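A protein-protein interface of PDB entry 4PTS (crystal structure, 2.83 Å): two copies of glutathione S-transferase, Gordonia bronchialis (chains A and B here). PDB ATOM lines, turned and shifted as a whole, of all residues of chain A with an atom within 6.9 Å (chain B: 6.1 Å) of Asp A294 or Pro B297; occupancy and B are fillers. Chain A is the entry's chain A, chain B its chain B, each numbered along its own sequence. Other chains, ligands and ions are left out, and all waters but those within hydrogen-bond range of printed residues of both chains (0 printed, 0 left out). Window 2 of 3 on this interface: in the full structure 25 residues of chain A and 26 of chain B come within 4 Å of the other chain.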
ATOM      1  N   LYS A 250     -31.031 -16.631 -32.265  1.00  0.00           N
ATOM      2  CA  LYS A 250     -30.613 -15.280 -31.864  1.00  0.00           C
ATOM      3  C   LYS A 250     -30.764 -14.223 -32.950  1.00  0.00           C
ATOM      4  O   LYS A 250     -30.002 -13.272 -32.990  1.00  0.00           O
ATOM      5  CB  LYS A 250     -29.172 -15.296 -31.375  1.00  0.00           C
ATOM      6  CG  LYS A 250     -28.964 -16.155 -30.149  1.00  0.00           C
ATOM      7  CD  LYS A 250     -27.500 -16.167 -29.743  1.00  0.00           C
ATOM      8  CE  LYS A 250     -27.253 -16.905 -28.434  1.00  0.00           C
ATOM      9  NZ  LYS A 250     -27.023 -18.345 -28.688  1.00  0.00           N
ATOM     10  N   ILE A 290     -35.043 -29.323 -29.201  1.00  0.00           N
ATOM     11  CA  ILE A 290     -34.570 -30.595 -28.692  1.00  0.00           C
ATOM     12  C   ILE A 290     -33.456 -31.171 -29.551  1.00  0.00           C
ATOM     13  O   ILE A 290     -32.497 -31.692 -28.995  1.00  0.00           O
ATOM     14  CB  ILE A 290     -35.707 -31.612 -28.535  1.00  0.00           C
ATOM     15  CG1 ILE A 290     -36.654 -31.154 -27.422  1.00  0.00           C
ATOM     16  CG2 ILE A 290     -35.161 -32.984 -28.189  1.00  0.00           C
ATOM     17  CD1 ILE A 290     -38.039 -31.782 -27.487  1.00  0.00           C
ATOM     18  N   VAL A 291     -33.539 -31.107 -30.878  1.00  0.00           N
ATOM     19  CA  VAL A 291     -32.520 -31.798 -31.681  1.00  0.00           C
ATOM     20  C   VAL A 291     -31.167 -31.082 -31.619  1.00  0.00           C
ATOM     21  O   VAL A 291     -30.143 -31.734 -31.518  1.00  0.00           O
ATOM     22  CB  VAL A 291     -32.960 -32.059 -33.138  1.00  0.00           C
ATOM     23  CG1 VAL A 291     -31.802 -32.561 -33.990  1.00  0.00           C
ATOM     24  CG2 VAL A 291     -34.101 -33.069 -33.174  1.00  0.00           C
ATOM     25  N   HIS A 292     -31.173 -29.759 -31.626  1.00  0.00           N
ATOM     26  CA  HIS A 292     -29.944 -28.960 -31.570  1.00  0.00           C
ATOM     27  C   HIS A 292     -29.392 -28.761 -30.149  1.00  0.00           C
ATOM     28  O   HIS A 292     -29.344 -27.646 -29.632  1.00  0.00           O
ATOM     29  CB  HIS A 292     -30.216 -27.591 -32.174  1.00  0.00           C
ATOM     30  CG  HIS A 292     -30.631 -27.638 -33.604  1.00  0.00           C
ATOM     31  ND1 HIS A 292     -31.529 -26.750 -34.154  1.00  0.00           N
ATOM     32  CD2 HIS A 292     -30.272 -28.478 -34.602  1.00  0.00           C
ATOM     33  CE1 HIS A 292     -31.691 -27.029 -35.438  1.00  0.00           C
ATOM     34  NE2 HIS A 292     -30.945 -28.076 -35.734  1.00  0.00           N
ATOM     35  N   SER A 293     -28.932 -29.846 -29.541  1.00  0.00           N
ATOM     36  CA  SER A 293     -28.395 -29.841 -28.164  1.00  0.00           C
ATOM     37  C   SER A 293     -27.087 -29.072 -28.030  1.00  0.00           C
ATOM     38  O   SER A 293     -26.700 -28.656 -26.954  1.00  0.00           O
ATOM     39  CB  SER A 293     -28.128 -31.273 -27.724  1.00  0.00           C
ATOM     40  OG  SER A 293     -28.945 -32.160 -28.462  1.00  0.00           O
ATOM     41  N   ASP A 294     -26.387 -28.948 -29.137  1.00  0.00           N
ATOM     42  CA  ASP A 294     -25.159 -28.212 -29.167  1.00  0.00           C
ATOM     43  C   ASP A 294     -25.399 -26.737 -28.955  1.00  0.00           C
ATOM     44  O   ASP A 294     -24.585 -26.079 -28.339  1.00  0.00           O
ATOM     45  CB  ASP A 294     -24.444 -28.475 -30.487  1.00  0.00           C
ATOM     46  CG  ASP A 294     -23.938 -29.929 -30.589  1.00  0.00           C
ATOM     47  OD1 ASP A 294     -23.622 -30.557 -29.528  1.00  0.00           O
ATOM     48  OD2 ASP A 294     -23.863 -30.445 -31.737  1.00  0.00           O
ATOM     49  N   ILE A 295     -26.513 -26.218 -29.452  1.00  0.00           N
ATOM     50  CA  ILE A 295     -26.858 -24.835 -29.212  1.00  0.00           C
ATOM     51  C   ILE A 295     -27.676 -24.644 -27.929  1.00  0.00           C
ATOM     52  O   ILE A 295     -27.572 -23.608 -27.261  1.00  0.00           O
ATOM     53  CB  ILE A 295     -27.665 -24.299 -30.387  1.00  0.00           C
ATOM     54  CG1 ILE A 295     -26.753 -24.133 -31.583  1.00  0.00           C
ATOM     55  CG2 ILE A 295     -28.305 -22.950 -30.065  1.00  0.00           C
ATOM     56  CD1 ILE A 295     -27.519 -23.771 -32.845  1.00  0.00           C
ATOM     57  N   ASN A 296     -28.526 -25.623 -27.614  1.00  0.00           N
ATOM     58  CA  ASN A 296     -29.442 -25.547 -26.473  1.00  0.00           C
ATOM     59  C   ASN A 296     -29.399 -26.826 -25.673  1.00  0.00           C
ATOM     60  O   ASN A 296     -30.290 -27.655 -25.797  1.00  0.00           O
ATOM     61  CB  ASN A 296     -30.862 -25.341 -26.962  1.00  0.00           C
ATOM     62  CG  ASN A 296     -31.857 -25.349 -25.827  1.00  0.00           C
ATOM     63  OD1 ASN A 296     -31.586 -24.796 -24.762  1.00  0.00           O
ATOM     64  ND2 ASN A 296     -33.002 -25.984 -26.036  1.00  0.00           N
ATOM     65  N   PRO A 297     -28.360 -26.997 -24.846  1.00  0.00           N
ATOM     66  CA  PRO A 297     -28.140 -28.274 -24.192  1.00  0.00           C
ATOM     67  C   PRO A 297     -29.153 -28.646 -23.099  1.00  0.00           C
ATOM     68  O   PRO A 297     -29.307 -29.823 -22.831  1.00  0.00           O
ATOM     69  CB  PRO A 297     -26.735 -28.158 -23.640  1.00  0.00           C
ATOM     70  CG  PRO A 297     -26.466 -26.712 -23.537  1.00  0.00           C
ATOM     71  CD  PRO A 297     -27.322 -26.009 -24.526  1.00  0.00           C
ATOM     72  N   HIS B 292     -22.744 -17.687 -18.694  1.00  0.00           N
ATOM     73  CA  HIS B 292     -23.598 -18.877 -18.588  1.00  0.00           C
ATOM     74  C   HIS B 292     -23.429 -19.858 -19.739  1.00  0.00           C
ATOM     75  O   HIS B 292     -24.349 -20.079 -20.517  1.00  0.00           O
ATOM     76  CB  HIS B 292     -25.047 -18.456 -18.525  1.00  0.00           C
ATOM     77  CG  HIS B 292     -25.376 -17.627 -17.330  1.00  0.00           C
ATOM     78  ND1 HIS B 292     -26.335 -16.635 -17.345  1.00  0.00           N
ATOM     79  CD2 HIS B 292     -24.894 -17.670 -16.069  1.00  0.00           C
ATOM     80  CE1 HIS B 292     -26.425 -16.097 -16.145  1.00  0.00           C
ATOM     81  NE2 HIS B 292     -25.556 -16.701 -15.353  1.00  0.00           N
ATOM     82  N   SER B 293     -22.240 -20.453 -19.816  1.00  0.00           N
ATOM     83  CA  SER B 293     -21.842 -21.348 -20.903  1.00  0.00           C
ATOM     84  C   SER B 293     -22.615 -22.661 -20.864  1.00  0.00           C
ATOM     85  O   SER B 293     -22.761 -23.340 -21.887  1.00  0.00           O
ATOM     86  CB  SER B 293     -20.343 -21.626 -20.785  1.00  0.00           C
ATOM     87  OG  SER B 293     -20.073 -22.247 -19.532  1.00  0.00           O
ATOM     88  N   ASP B 294     -23.110 -23.015 -19.686  1.00  0.00           N
ATOM     89  CA  ASP B 294     -23.917 -24.204 -19.535  1.00  0.00           C
ATOM     90  C   ASP B 294     -25.274 -24.048 -20.252  1.00  0.00           C
ATOM     91  O   ASP B 294     -25.780 -25.008 -20.808  1.00  0.00           O
ATOM     92  CB  ASP B 294     -24.058 -24.617 -18.047  1.00  0.00           C
ATOM     93  CG  ASP B 294     -24.635 -23.492 -17.142  1.00  0.00           C
ATOM     94  OD1 ASP B 294     -24.355 -22.274 -17.362  1.00  0.00           O
ATOM     95  OD2 ASP B 294     -25.362 -23.849 -16.178  1.00  0.00           O
ATOM     96  N   ILE B 295     -25.839 -22.845 -20.282  1.00  0.00           N
ATOM     97  CA  ILE B 295     -27.073 -22.592 -21.027  1.00  0.00           C
ATOM     98  C   ILE B 295     -26.819 -22.183 -22.482  1.00  0.00           C
ATOM     99  O   ILE B 295     -27.611 -22.493 -23.372  1.00  0.00           O
ATOM    100  CB  ILE B 295     -27.859 -21.486 -20.357  1.00  0.00           C
ATOM    101  CG1 ILE B 295     -28.428 -22.006 -19.056  1.00  0.00           C
ATOM    102  CG2 ILE B 295     -28.995 -20.988 -21.236  1.00  0.00           C
ATOM    103  CD1 ILE B 295     -29.091 -20.907 -18.237  1.00  0.00           C
ATOM    104  N   ASN B 296     -25.719 -21.473 -22.713  1.00  0.00           N
ATOM    105  CA  ASN B 296     -25.395 -20.951 -24.029  1.00  0.00           C
ATOM    106  C   ASN B 296     -23.942 -21.199 -24.350  1.00  0.00           C
ATOM    107  O   ASN B 296     -23.128 -20.293 -24.256  1.00  0.00           O
ATOM    108  CB  ASN B 296     -25.648 -19.441 -24.066  1.00  0.00           C
ATOM    109  CG  ASN B 296     -25.281 -18.831 -25.393  1.00  0.00           C
ATOM    110  OD1 ASN B 296     -25.515 -19.432 -26.438  1.00  0.00           O
ATOM    111  ND2 ASN B 296     -24.659 -17.664 -25.363  1.00  0.00           N
ATOM    112  N   PRO B 297     -23.623 -22.419 -24.774  1.00  0.00           N
ATOM    113  CA  PRO B 297     -22.223 -22.797 -24.927  1.00  0.00           C
ATOM    114  C   PRO B 297     -21.485 -22.145 -26.089  1.00  0.00           C
ATOM    115  O   PRO B 297     -20.277 -22.066 -26.044  1.00  0.00           O
ATOM    116  CB  PRO B 297     -22.272 -24.311 -25.064  1.00  0.00           C
ATOM    117  CG  PRO B 297     -23.645 -24.631 -25.490  1.00  0.00           C
ATOM    118  CD  PRO B 297     -24.546 -23.527 -25.051  1.00  0.00           C
ATOM    119  N   THR B 298     -22.175 -21.672 -27.118  1.00  0.00           N
ATOM    120  CA  THR B 298     -21.475 -20.901 -28.158  1.00  0.00           C
ATOM    121  C   THR B 298     -20.886 -19.607 -27.601  1.00  0.00           C
ATOM    122  O   THR B 298     -19.959 -19.062 -28.187  1.00  0.00           O
ATOM    123  CB  THR B 298     -22.374 -20.527 -29.379  1.00  0.00           C
ATOM    124  OG1 THR B 298     -23.538 -19.778 -28.960  1.00  0.00           O
ATOM    125  CG2 THR B 298     -22.783 -21.767 -30.151  1.00  0.00           C
ATOM    126  N   GLN B 299     -21.467 -19.099 -26.509  1.00  0.00           N
ATOM    127  CA  GLN B 299     -21.066 -17.817 -25.904  1.00  0.00           C
ATOM    128  C   GLN B 299     -21.133 -16.666 -26.888  1.00  0.00           C
ATOM    129  O   GLN B 299     -20.430 -15.654 -26.757  1.00  0.00           O
ATOM    130  CB  GLN B 299     -19.672 -17.893 -25.295  1.00  0.00           C
ATOM    131  CG  GLN B 299     -19.496 -19.061 -24.361  1.00  0.00           C
ATOM    132  CD  GLN B 299     -18.149 -19.047 -23.692  1.00  0.00           C
ATOM    133  OE1 GLN B 299     -17.186 -19.659 -24.177  1.00  0.00           O
ATOM    134  NE2 GLN B 299     -18.062 -18.342 -22.581  1.00  0.00           N
ATOM    135  N   ILE B 300     -22.022 -16.814 -27.858  1.00  0.00           N
ATOM    136  CA  ILE B 300     -22.298 -15.750 -28.793  1.00  0.00           C
ATOM    137  C   ILE B 300     -23.335 -14.825 -28.178  1.00  0.00           C
ATOM    138  O   ILE B 300     -24.312 -15.269 -27.591  1.00  0.00           O
ATOM    139  CB  ILE B 300     -22.801 -16.321 -30.105  1.00  0.00           C
ATOM    140  CG1 ILE B 300     -21.656 -17.055 -30.778  1.00  0.00           C
ATOM    141  CG2 ILE B 300     -23.325 -15.214 -31.015  1.00  0.00           C
ATOM    142  CD1 ILE B 300     -22.067 -17.697 -32.084  1.00  0.00           C
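OD1 of Asn B296 sits at hydrogen-bond distance from NZ of Lys A250, 2.9 Å away.
OD1 of Asn B296 is in hydrogen-bond range of OG1 of Thr B298 (3.2 Å).
O of Ile B300 lies within hydrogen-bond range of ND2 of Asn B296, 3.3 Å away.
Among the printed residues, pairs that only touch across the chains: Pro A297 with Asp B294 (3.3 Å), Asp A294 with Pro B297 (3.3 Å), Lys A250 with Ile B300 (3.5 Å), Pro A297 with Ile B295 (3.7 Å), Ile A295 with Pro B297 (3.7 Å), Pro A297 with Pro B297 (3.8 Å) and Lys A250 with Thr B298 (3.8 Å).
Of the printed residues of chain B, Lys A250 touches Asn B296 (2.9 Å), Thr B298 (3.8 Å) and Ile B300 (3.5 Å).
Asp A294 touches one residue of chain B.
Of the printed residues of chain B, Ile A295 touches Pro B297.
Of the printed residues of chain B, Pro A297 touches Asp B294, Ile B295 and Pro B297.
Printed residues of chain A within 4 Å of Pro B297: Asp A294 (3.3 Å), Ile A295 (3.7 Å) and Pro A297 (3.8 Å).
Printed residues of chain A within 4 Å of Thr B298: Lys A250 (3.8 Å).
Gln B299 touches none of the printed residues of chain A.
The nearest residue of chain B that does not touch Asp A294 is Thr B298 (5.0 Å).
The nearest printed residue of chain A that does not touch Thr B298 is Ile A295 (4.8 Å).
Of the 9 printed residues of chain A, 4 touch a printed residue of chain B.
Hydrophobic or aromatic side chains of chain A that line the printed part of chain B: Pro A297.
Among the printed residues, no Asp or Glu carboxylate lies within 4 Å of a Lys or Arg side-chain nitrogen of the other chain.
Asp A294 touches Pro B297, and with the chains exchanged Pro A297 touches Asp B294.
Ile A295 touches Pro B297, and with the chains exchanged Pro A297 touches Ile B295.
Pro B297 touches its own counterpart, Pro A297.
Of the 8 pairs that touch across the chains among the printed residues, 5 have their exchanged pair printed and touching as well.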
